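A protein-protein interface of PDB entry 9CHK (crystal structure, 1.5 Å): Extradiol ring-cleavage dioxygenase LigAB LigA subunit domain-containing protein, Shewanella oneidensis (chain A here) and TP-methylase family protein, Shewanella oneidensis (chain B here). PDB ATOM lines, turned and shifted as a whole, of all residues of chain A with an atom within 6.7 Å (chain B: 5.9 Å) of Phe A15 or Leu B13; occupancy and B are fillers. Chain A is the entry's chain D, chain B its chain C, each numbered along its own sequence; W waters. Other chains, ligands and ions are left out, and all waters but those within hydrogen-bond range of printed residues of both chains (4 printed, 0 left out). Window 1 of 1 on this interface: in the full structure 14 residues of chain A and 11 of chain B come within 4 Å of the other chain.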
ATOM      1  N   GLY A  10     -25.824  16.000  -7.250  1.00  0.00           N
ATOM      2  CA  GLY A  10     -26.321  15.768  -8.598  1.00  0.00           C
ATOM      3  C   GLY A  10     -26.003  14.360  -9.099  1.00  0.00           C
ATOM      4  O   GLY A  10     -26.842  13.724  -9.734  1.00  0.00           O
ATOM      5  N   LEU A  11     -24.778  13.895  -8.829  1.00  0.00           N
ATOM      6  CA  LEU A  11     -24.335  12.580  -9.266  1.00  0.00           C
ATOM      7  C   LEU A  11     -25.268  11.530  -8.668  1.00  0.00           C
ATOM      8  O   LEU A  11     -25.808  10.672  -9.372  1.00  0.00           O
ATOM      9  CB  LEU A  11     -22.896  12.357  -8.803  1.00  0.00           C
ATOM     10  CG  LEU A  11     -21.958  11.646  -9.785  1.00  0.00           C
ATOM     11  CD1 LEU A  11     -21.005  10.731  -9.032  1.00  0.00           C
ATOM     12  CD2 LEU A  11     -22.690  10.885 -10.874  1.00  0.00           C
ATOM     13  N   SER A  12     -25.445  11.632  -7.347  1.00  0.00           N
ATOM     14  CA  SER A  12     -26.238  10.694  -6.574  1.00  0.00           C
ATOM     15  C   SER A  12     -27.697  10.726  -7.024  1.00  0.00           C
ATOM     16  O   SER A  12     -28.321   9.679  -7.165  1.00  0.00           O
ATOM     17  CB  SER A  12     -26.113  10.988  -5.097  1.00  0.00           C
ATOM     18  OG  SER A  12     -26.978  10.157  -4.335  1.00  0.00           O
ATOM     19  N   ASP A  13     -28.234  11.933  -7.236  1.00  0.00           N
ATOM     20  CA  ASP A  13     -29.620  12.098  -7.640  1.00  0.00           C
ATOM     21  C   ASP A  13     -29.845  11.401  -8.979  1.00  0.00           C
ATOM     22  O   ASP A  13     -30.865  10.736  -9.173  1.00  0.00           O
ATOM     23  CB  ASP A  13     -30.005  13.569  -7.709  1.00  0.00           C
ATOM     24  CG  ASP A  13     -30.048  14.311  -6.381  1.00  0.00           C
ATOM     25  OD1 ASP A  13     -30.049  13.640  -5.330  1.00  0.00           O
ATOM     26  OD2 ASP A  13     -30.066  15.560  -6.410  1.00  0.00           O
ATOM     27  N   PHE A  14     -28.880  11.567  -9.893  1.00  0.00           N
ATOM     28  CA  PHE A  14     -28.951  10.973 -11.218  1.00  0.00           C
ATOM     29  C   PHE A  14     -28.974   9.450 -11.096  1.00  0.00           C
ATOM     30  O   PHE A  14     -29.832   8.794 -11.679  1.00  0.00           O
ATOM     31  CB  PHE A  14     -27.776  11.415 -12.095  1.00  0.00           C
ATOM     32  CG  PHE A  14     -27.713  10.713 -13.442  1.00  0.00           C
ATOM     33  CD1 PHE A  14     -28.792  10.752 -14.319  1.00  0.00           C
ATOM     34  CD2 PHE A  14     -26.599   9.964 -13.802  1.00  0.00           C
ATOM     35  CE1 PHE A  14     -28.737  10.097 -15.539  1.00  0.00           C
ATOM     36  CE2 PHE A  14     -26.552   9.307 -15.023  1.00  0.00           C
ATOM     37  CZ  PHE A  14     -27.621   9.374 -15.886  1.00  0.00           C
ATOM     38  N   PHE A  15     -28.026   8.888 -10.339  1.00  0.00           N
ATOM     39  CA  PHE A  15     -27.926   7.440 -10.234  1.00  0.00           C
ATOM     40  C   PHE A  15     -29.198   6.873  -9.606  1.00  0.00           C
ATOM     41  O   PHE A  15     -29.670   5.813 -10.008  1.00  0.00           O
ATOM     42  CB  PHE A  15     -26.697   6.984  -9.442  1.00  0.00           C
ATOM     43  CG  PHE A  15     -25.362   7.190 -10.142  1.00  0.00           C
ATOM     44  CD1 PHE A  15     -25.294   7.434 -11.508  1.00  0.00           C
ATOM     45  CD2 PHE A  15     -24.172   7.133  -9.424  1.00  0.00           C
ATOM     46  CE1 PHE A  15     -24.070   7.625 -12.135  1.00  0.00           C
ATOM     47  CE2 PHE A  15     -22.953   7.315 -10.057  1.00  0.00           C
ATOM     48  CZ  PHE A  15     -22.906   7.560 -11.410  1.00  0.00           C
ATOM     49  N   THR A  16     -29.756   7.574  -8.614  1.00  0.00           N
ATOM     50  CA  THR A  16     -30.954   7.082  -7.951  1.00  0.00           C
ATOM     51  C   THR A  16     -32.118   7.053  -8.942  1.00  0.00           C
ATOM     52  O   THR A  16     -32.894   6.099  -8.965  1.00  0.00           O
ATOM     53  CB  THR A  16     -31.280   7.927  -6.719  1.00  0.00           C
ATOM     54  OG1 THR A  16     -30.304   7.590  -5.738  1.00  0.00           O
ATOM     55  CG2 THR A  16     -32.663   7.637  -6.169  1.00  0.00           C
ATOM     56  N   GLN A  17     -32.247   8.096  -9.770  1.00  0.00           N
ATOM     57  CA  GLN A  17     -33.355   8.142 -10.709  1.00  0.00           C
ATOM     58  C   GLN A  17     -33.151   7.077 -11.785  1.00  0.00           C
ATOM     59  O   GLN A  17     -34.080   6.344 -12.123  1.00  0.00           O
ATOM     60  CB  GLN A  17     -33.572   9.504 -11.366  1.00  0.00           C
ATOM     61  CG  GLN A  17     -34.846   9.551 -12.202  1.00  0.00           C
ATOM     62  CD  GLN A  17     -35.040  10.841 -12.967  1.00  0.00           C
ATOM     63  OE1 GLN A  17     -34.244  11.782 -12.875  1.00  0.00           O
ATOM     64  NE2 GLN A  17     -36.116  10.892 -13.741  1.00  0.00           N
ATOM     65  N   LEU A  18     -31.925   6.982 -12.310  1.00  0.00           N
ATOM     66  CA  LEU A  18     -31.621   6.033 -13.369  1.00  0.00           C
ATOM     67  C   LEU A  18     -31.951   4.616 -12.903  1.00  0.00           C
ATOM     68  O   LEU A  18     -32.452   3.796 -13.674  1.00  0.00           O
ATOM     69  CB  LEU A  18     -30.150   6.180 -13.758  1.00  0.00           C
ATOM     70  CG  LEU A  18     -29.643   5.240 -14.855  1.00  0.00           C
ATOM     71  CD1 LEU A  18     -30.410   5.476 -16.141  1.00  0.00           C
ATOM     72  CD2 LEU A  18     -28.150   5.429 -15.084  1.00  0.00           C
ATOM     73  N   GLY A  19     -31.689   4.344 -11.622  1.00  0.00           N
ATOM     74  CA  GLY A  19     -31.808   3.004 -11.078  1.00  0.00           C
ATOM     75  C   GLY A  19     -33.257   2.535 -10.974  1.00  0.00           C
ATOM     76  O   GLY A  19     -33.493   1.334 -10.880  1.00  0.00           O
ATOM     77  N   GLN A  20     -34.223   3.466 -10.964  1.00  0.00           N
ATOM     78  CA  GLN A  20     -35.595   3.064 -10.680  1.00  0.00           C
ATOM     79  C   GLN A  20     -36.563   3.464 -11.794  1.00  0.00           C
ATOM     80  O   GLN A  20     -37.716   3.042 -11.771  1.00  0.00           O
ATOM     81  CB  GLN A  20     -36.073   3.569  -9.320  1.00  0.00           C
ATOM     82  CG  GLN A  20     -35.962   5.074  -9.117  1.00  0.00           C
ATOM     83  CD  GLN A  20     -36.201   5.462  -7.674  1.00  0.00           C
ATOM     84  OE1 GLN A  20     -37.208   5.084  -7.064  1.00  0.00           O
ATOM     85  NE2 GLN A  20     -35.256   6.189  -7.102  1.00  0.00           N
ATOM     86  N   MET A  36     -25.898  11.453 -19.724  1.00  0.00           N
ATOM     87  CA  MET A  36     -25.089  11.882 -18.593  1.00  0.00           C
ATOM     88  C   MET A  36     -24.765  13.372 -18.699  1.00  0.00           C
ATOM     89  O   MET A  36     -24.811  14.086 -17.697  1.00  0.00           O
ATOM     90  CB  MET A  36     -23.806  11.055 -18.484  1.00  0.00           C
ATOM     91  CG  MET A  36     -24.060   9.665 -17.945  1.00  0.00           C
ATOM     92  SD  MET A  36     -22.550   8.744 -17.598  1.00  0.00           S
ATOM     93  CE  MET A  36     -22.141   8.149 -19.244  1.00  0.00           C
ATOM     94  N   LEU A  41     -23.424  15.701 -15.480  1.00  0.00           N
ATOM     95  CA  LEU A  41     -22.198  15.029 -15.076  1.00  0.00           C
ATOM     96  C   LEU A  41     -21.000  15.726 -15.722  1.00  0.00           C
ATOM     97  O   LEU A  41     -21.096  16.209 -16.848  1.00  0.00           O
ATOM     98  CB  LEU A  41     -22.237  13.540 -15.420  1.00  0.00           C
ATOM     99  CG  LEU A  41     -22.900  12.631 -14.378  1.00  0.00           C
ATOM    100  CD1 LEU A  41     -24.367  12.967 -14.181  1.00  0.00           C
ATOM    101  CD2 LEU A  41     -22.740  11.171 -14.748  1.00  0.00           C
ATOM    102  N   GLN A  45     -16.463  12.674 -14.436  1.00  0.00           N
ATOM    103  CA  GLN A  45     -17.454  11.720 -13.961  1.00  0.00           C
ATOM    104  C   GLN A  45     -17.805  10.753 -15.089  1.00  0.00           C
ATOM    105  O   GLN A  45     -17.875   9.544 -14.876  1.00  0.00           O
ATOM    106  CB  GLN A  45     -18.684  12.455 -13.427  1.00  0.00           C
ATOM    107  CG  GLN A  45     -18.479  13.062 -12.041  1.00  0.00           C
ATOM    108  CD  GLN A  45     -19.595  13.991 -11.613  1.00  0.00           C
ATOM    109  OE1 GLN A  45     -20.447  14.400 -12.410  1.00  0.00           O
ATOM    110  NE2 GLN A  45     -19.588  14.349 -10.337  1.00  0.00           N
ATOM    111  N   VAL A  49     -17.231   6.628 -15.535  1.00  0.00           N
ATOM    112  CA  VAL A  49     -18.311   5.711 -15.855  1.00  0.00           C
ATOM    113  C   VAL A  49     -17.869   4.835 -17.023  1.00  0.00           C
ATOM    114  O   VAL A  49     -18.014   3.615 -16.981  1.00  0.00           O
ATOM    115  CB  VAL A  49     -19.630   6.434 -16.185  1.00  0.00           C
ATOM    116  CG1 VAL A  49     -20.626   5.504 -16.868  1.00  0.00           C
ATOM    117  CG2 VAL A  49     -20.255   7.069 -14.950  1.00  0.00           C
ATOM    118  N   LEU A  57     -15.432   7.342  -9.147  1.00  0.00           N
ATOM    119  CA  LEU A  57     -16.793   7.851  -9.088  1.00  0.00           C
ATOM    120  C   LEU A  57     -17.152   8.231  -7.654  1.00  0.00           C
ATOM    121  O   LEU A  57     -17.722   9.293  -7.418  1.00  0.00           O
ATOM    122  CB  LEU A  57     -17.793   6.835  -9.634  1.00  0.00           C
ATOM    123  CG  LEU A  57     -18.178   6.991 -11.106  1.00  0.00           C
ATOM    124  CD1 LEU A  57     -19.259   5.982 -11.456  1.00  0.00           C
ATOM    125  CD2 LEU A  57     -18.635   8.410 -11.410  1.00  0.00           C
ATOM    126  N   LEU B  11     -29.297  -5.717  -4.982  1.00  0.00           N
ATOM    127  CA  LEU B  11     -27.898  -5.374  -5.181  1.00  0.00           C
ATOM    128  C   LEU B  11     -27.761  -4.030  -5.894  1.00  0.00           C
ATOM    129  O   LEU B  11     -26.825  -3.278  -5.607  1.00  0.00           O
ATOM    130  CB  LEU B  11     -27.185  -6.492  -5.938  1.00  0.00           C
ATOM    131  CG  LEU B  11     -26.890  -7.756  -5.123  1.00  0.00           C
ATOM    132  CD1 LEU B  11     -26.091  -8.753  -5.937  1.00  0.00           C
ATOM    133  CD2 LEU B  11     -26.166  -7.413  -3.832  1.00  0.00           C
ATOM    134  N   GLN B  12     -28.672  -3.746  -6.832  1.00  0.00           N
ATOM    135  CA  GLN B  12     -28.637  -2.509  -7.598  1.00  0.00           C
ATOM    136  C   GLN B  12     -29.280  -1.375  -6.804  1.00  0.00           C
ATOM    137  O   GLN B  12     -30.272  -1.578  -6.112  1.00  0.00           O
ATOM    138  CB  GLN B  12     -29.365  -2.642  -8.936  1.00  0.00           C
ATOM    139  CG  GLN B  12     -28.480  -3.108 -10.087  1.00  0.00           C
ATOM    140  CD  GLN B  12     -27.505  -2.044 -10.545  1.00  0.00           C
ATOM    141  OE1 GLN B  12     -27.430  -0.949  -9.973  1.00  0.00           O
ATOM    142  NE2 GLN B  12     -26.748  -2.357 -11.584  1.00  0.00           N
ATOM    143  N   LEU B  13     -28.700  -0.177  -6.939  1.00  0.00           N
ATOM    144  CA  LEU B  13     -29.186   1.028  -6.287  1.00  0.00           C
ATOM    145  C   LEU B  13     -30.637   1.320  -6.665  1.00  0.00           C
ATOM    146  O   LEU B  13     -30.978   1.397  -7.844  1.00  0.00           O
ATOM    147  CB  LEU B  13     -28.263   2.174  -6.701  1.00  0.00           C
ATOM    148  CG  LEU B  13     -28.709   3.578  -6.282  1.00  0.00           C
ATOM    149  CD1 LEU B  13     -28.590   3.755  -4.777  1.00  0.00           C
ATOM    150  CD2 LEU B  13     -27.900   4.620  -7.032  1.00  0.00           C
ATOM    151  N   ALA B  14     -31.470   1.470  -5.625  1.00  0.00           N
ATOM    152  CA  ALA B  14     -32.771   2.124  -5.684  1.00  0.00           C
ATOM    153  C   ALA B  14     -33.852   1.251  -6.321  1.00  0.00           C
ATOM    154  O   ALA B  14     -34.975   1.221  -5.824  1.00  0.00           O
ATOM    155  CB  ALA B  14     -32.661   3.460  -6.395  1.00  0.00           C
ATOM    156  N   GLY B  15     -33.538   0.573  -7.428  1.00  0.00           N
ATOM    157  CA  GLY B  15     -34.572  -0.020  -8.262  1.00  0.00           C
ATOM    158  C   GLY B  15     -34.857  -1.493  -7.967  1.00  0.00           C
ATOM    159  O   GLY B  15     -35.837  -2.040  -8.474  1.00  0.00           O
ATOM    160  N   GLN B  16     -34.013  -2.147  -7.169  1.00  0.00           N
ATOM    161  CA  GLN B  16     -34.103  -3.592  -7.035  1.00  0.00           C
ATOM    162  C   GLN B  16     -34.809  -3.990  -5.742  1.00  0.00           C
ATOM    163  O   GLN B  16     -34.981  -5.178  -5.484  1.00  0.00           O
ATOM    164  CB  GLN B  16     -32.716  -4.219  -7.141  1.00  0.00           C
ATOM    165  CG  GLN B  16     -32.731  -5.633  -7.704  1.00  0.00           C
ATOM    166  CD  GLN B  16     -31.381  -6.051  -8.236  1.00  0.00           C
ATOM    167  OE1 GLN B  16     -30.374  -5.991  -7.525  1.00  0.00           O
ATOM    168  NE2 GLN B  16     -31.345  -6.456  -9.499  1.00  0.00           N
ATOM    169  N   ASP B  37     -22.789   0.866  -0.479  1.00  0.00           N
ATOM    170  CA  ASP B  37     -22.009   2.054  -0.792  1.00  0.00           C
ATOM    171  C   ASP B  37     -22.741   3.325  -0.363  1.00  0.00           C
ATOM    172  O   ASP B  37     -23.871   3.271   0.116  1.00  0.00           O
ATOM    173  CB  ASP B  37     -21.694   2.118  -2.278  1.00  0.00           C
ATOM    174  CG  ASP B  37     -22.914   2.105  -3.187  1.00  0.00           C
ATOM    175  OD1 ASP B  37     -23.863   2.855  -2.891  1.00  0.00           O
ATOM    176  OD2 ASP B  37     -22.901   1.356  -4.187  1.00  0.00           O
ATOM    177  N   PHE B  39     -23.870   5.753  -2.237  1.00  0.00           N
ATOM    178  CA  PHE B  39     -25.008   6.090  -3.079  1.00  0.00           C
ATOM    179  C   PHE B  39     -26.282   5.475  -2.504  1.00  0.00           C
ATOM    180  O   PHE B  39     -27.318   6.138  -2.436  1.00  0.00           O
ATOM    181  CB  PHE B  39     -24.800   5.647  -4.529  1.00  0.00           C
ATOM    182  CG  PHE B  39     -23.659   6.380  -5.220  1.00  0.00           C
ATOM    183  CD1 PHE B  39     -23.812   7.696  -5.639  1.00  0.00           C
ATOM    184  CD2 PHE B  39     -22.440   5.753  -5.449  1.00  0.00           C
ATOM    185  CE1 PHE B  39     -22.771   8.368  -6.259  1.00  0.00           C
ATOM    186  CE2 PHE B  39     -21.404   6.431  -6.070  1.00  0.00           C
ATOM    187  CZ  PHE B  39     -21.574   7.731  -6.481  1.00  0.00           C
ATOM    188  N   SER B  40     -26.213   4.199  -2.116  1.00  0.00           N
ATOM    189  CA  SER B  40     -27.375   3.531  -1.554  1.00  0.00           C
ATOM    190  C   SER B  40     -27.682   4.121  -0.180  1.00  0.00           C
ATOM    191  O   SER B  40     -28.843   4.258   0.190  1.00  0.00           O
ATOM    192  CB  SER B  40     -27.198   2.031  -1.507  1.00  0.00           C
ATOM    193  OG  SER B  40     -25.956   1.667  -0.924  1.00  0.00           O
ATOM    194  N   GLN B  41     -26.636   4.517   0.554  1.00  0.00           N
ATOM    195  CA  GLN B  41     -26.829   5.098   1.871  1.00  0.00           C
ATOM    196  C   GLN B  41     -27.625   6.398   1.760  1.00  0.00           C
ATOM    197  O   GLN B  41     -28.518   6.647   2.569  1.00  0.00           O
ATOM    198  CB  GLN B  41     -25.516   5.347   2.611  1.00  0.00           C
ATOM    199  CG  GLN B  41     -25.720   5.518   4.112  1.00  0.00           C
ATOM    200  CD  GLN B  41     -26.195   4.244   4.778  1.00  0.00           C
ATOM    201  OE1 GLN B  41     -25.907   3.134   4.319  1.00  0.00           O
ATOM    202  NE2 GLN B  41     -26.906   4.388   5.888  1.00  0.00           N
ATOM    203  N   TRP B  43     -29.589   7.276  -0.770  1.00  0.00           N
ATOM    204  CA  TRP B  43     -30.911   6.891  -1.236  1.00  0.00           C
ATOM    205  C   TRP B  43     -31.802   6.516  -0.054  1.00  0.00           C
ATOM    206  O   TRP B  43     -32.959   6.922   0.013  1.00  0.00           O
ATOM    207  CB  TRP B  43     -30.800   5.736  -2.238  1.00  0.00           C
ATOM    208  CG  TRP B  43     -32.076   4.955  -2.399  1.00  0.00           C
ATOM    209  CD1 TRP B  43     -33.155   5.272  -3.168  1.00  0.00           C
ATOM    210  CD2 TRP B  43     -32.398   3.709  -1.745  1.00  0.00           C
ATOM    211  NE1 TRP B  43     -34.123   4.310  -3.049  1.00  0.00           N
ATOM    212  CE2 TRP B  43     -33.686   3.338  -2.187  1.00  0.00           C
ATOM    213  CE3 TRP B  43     -31.722   2.875  -0.849  1.00  0.00           C
ATOM    214  CZ2 TRP B  43     -34.310   2.174  -1.746  1.00  0.00           C
ATOM    215  CZ3 TRP B  43     -32.342   1.726  -0.414  1.00  0.00           C
ATOM    216  CH2 TRP B  43     -33.618   1.384  -0.857  1.00  0.00           C
ATOM    217  N   ALA B 209     -23.421  -5.894 -10.318  1.00  0.00           N
ATOM    218  CA  ALA B 209     -23.266  -4.451 -10.247  1.00  0.00           C
ATOM    219  C   ALA B 209     -24.129  -3.872  -9.128  1.00  0.00           C
ATOM    220  O   ALA B 209     -25.220  -4.369  -8.864  1.00  0.00           O
ATOM    221  CB  ALA B 209     -23.623  -3.835 -11.577  1.00  0.00           C
ATOM    222  N   ASN B 210     -23.628  -2.810  -8.485  1.00  0.00           N
ATOM    223  CA  ASN B 210     -24.372  -2.109  -7.449  1.00  0.00           C
ATOM    224  C   ASN B 210     -24.887  -0.762  -7.961  1.00  0.00           C
ATOM    225  O   ASN B 210     -25.745  -0.161  -7.319  1.00  0.00           O
ATOM    226  CB  ASN B 210     -23.536  -1.876  -6.193  1.00  0.00           C
ATOM    227  CG  ASN B 210     -23.140  -3.161  -5.506  1.00  0.00           C
ATOM    228  OD1 ASN B 210     -23.999  -3.928  -5.055  1.00  0.00           O
ATOM    229  ND2 ASN B 210     -21.844  -3.411  -5.411  1.00  0.00           N
ATOM    230  N   LEU B 211     -24.350  -0.280  -9.092  1.00  0.00           N
ATOM    231  CA  LEU B 211     -24.764   0.996  -9.662  1.00  0.00           C
ATOM    232  C   LEU B 211     -25.326   0.793 -11.067  1.00  0.00           C
ATOM    233  O   LEU B 211     -24.883  -0.091 -11.788  1.00  0.00           O
ATOM    234  CB  LEU B 211     -23.589   1.972  -9.688  1.00  0.00           C
ATOM    235  CG  LEU B 211     -23.085   2.449  -8.324  1.00  0.00           C
ATOM    236  CD1 LEU B 211     -21.874   3.347  -8.510  1.00  0.00           C
ATOM    237  CD2 LEU B 211     -24.173   3.164  -7.541  1.00  0.00           C
ATOM    238  N   PRO B 212     -26.301   1.626 -11.499  1.00  0.00           N
ATOM    239  CA  PRO B 212     -26.961   1.442 -12.794  1.00  0.00           C
ATOM    240  C   PRO B 212     -26.076   1.686 -14.014  1.00  0.00           C
ATOM    241  O   PRO B 212     -26.425   1.270 -15.116  1.00  0.00           O
ATOM    242  CB  PRO B 212     -28.134   2.436 -12.728  1.00  0.00           C
ATOM    243  CG  PRO B 212     -27.675   3.497 -11.756  1.00  0.00           C
ATOM    244  CD  PRO B 212     -26.853   2.749 -10.728  1.00  0.00           C
ATOM    245  N   ILE B 213     -24.932   2.349 -13.805  1.00  0.00           N
ATOM    246  CA  ILE B 213     -24.015   2.676 -14.886  1.00  0.00           C
ATOM    247  C   ILE B 213     -22.866   1.668 -14.914  1.00  0.00           C
ATOM    248  O   ILE B 213     -21.906   1.837 -15.661  1.00  0.00           O
ATOM    249  CB  ILE B 213     -23.496   4.123 -14.749  1.00  0.00           C
ATOM    250  CG1 ILE B 213     -22.903   4.396 -13.365  1.00  0.00           C
ATOM    251  CG2 ILE B 213     -24.585   5.138 -15.088  1.00  0.00           C
ATOM    252  CD1 ILE B 213     -21.689   3.553 -13.030  1.00  0.00           C
HETATM  253  O   HOH W   1     -36.099   6.741  -4.168  1.00  0.00           O
HETATM  254  O   HOH W   2     -36.441   3.356  -4.744  1.00  0.00           O
HETATM  255  O   HOH W   3     -27.586   7.621  -4.866  1.00  0.00           O
HETATM  256  O   HOH W   4     -19.237   1.832 -15.575  1.00  0.00           O
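Water W4 lies within hydrogen-bond range of O of Val A49 (2.6 Å) and O of Ile B213 (2.7 Å).
Water W3 lies within hydrogen-bond range of the side-chain hydroxyl of Ser A12 (2.7 Å), the side-chain hydroxyl of Thr A16 (2.9 Å) and the backbone carbonyl oxygen of Phe B39 (2.9 Å).
Water W2 lies within hydrogen-bond range of the backbone carbonyl oxygen of Ala B14 (2.8 Å), the side-chain amide oxygen of Gln A20 (3.0 Å) and the indole nitrogen of Trp B43 (3.0 Å).
Water W1 bridges NE2 of Gln A20 (3.1 Å) and NE1 of Trp B43 (3.3 Å).
The backbone carbonyl oxygen of Ser A12 lies within hydrogen-bond range of the side-chain hydroxyl of Thr A16.
O of Asn B210 is in hydrogen-bond range of N of Leu B13, at 3.0 Å.
The backbone carbonyl oxygen of Thr A16 is in hydrogen-bond range of the side-chain amide nitrogen of Gln A20 (3.0 Å).
OD1 of Asp B37 is in hydrogen-bond range of N of Phe B39.
Of the 16 printed residues of chain B, 7 touch a printed residue of chain A.
Hydrophobic or aromatic side chains of chain A that line the printed part of chain B: Leu A11, Phe A15, Leu A18, Val A49 and Leu A57.
Among the printed residues, 16 pairs touch across the chains.
Among the printed residues, no Asp or Glu carboxylate lies within 4 Å of a Lys or Arg side-chain nitrogen of the other chain.
Among the printed residues, merely in contact across the chains: Leu A11 with Phe B39 (3.98 Å), Ser A12 with Phe B39 (3.97 Å), Phe A15 with Leu B13 (3.6 Å), Phe A15 with Phe B39 (3.7 Å), Phe A15 with Pro B212 (3.5 Å), Phe A15 with Ile B213 (3.6 Å), Thr A16 with Leu B13 (3.8 Å), Thr A16 with Ala B14 (3.7 Å), Thr A16 with Trp B43 (3.9 Å), Leu A18 with Pro B212 (3.8 Å), Leu A18 with Ile B213 (3.6 Å), Gly A19 with Leu B13 (3.7 Å), Gly A19 with Gly B15 (3.1 Å), Gln A20 with Ala B14 (3.8 Å), Val A49 with Ile B213 (3.8 Å) and Leu A57 with Ile B213 (3.8 Å).
Phe A15 touches four residues of chain B.
Leu B13 touches three residues of chain A.
Printed residues of chain A within 4 Å of Gly B15: Gly A19.
Of the printed residues of chain B, Ser A12 touches Phe B39.
Of the printed residues of chain A, Trp B43 touches Thr A16 (3.9 Å).
Of the printed residues of chain B, Val A49 touches Ile B213 (3.8 Å).
The nearest residue of chain B that does not touch Phe A15 is Leu B211 (4.4 Å).
The nearest residue of chain A that does not touch Leu B13 is Gln A20 (5.0 Å).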
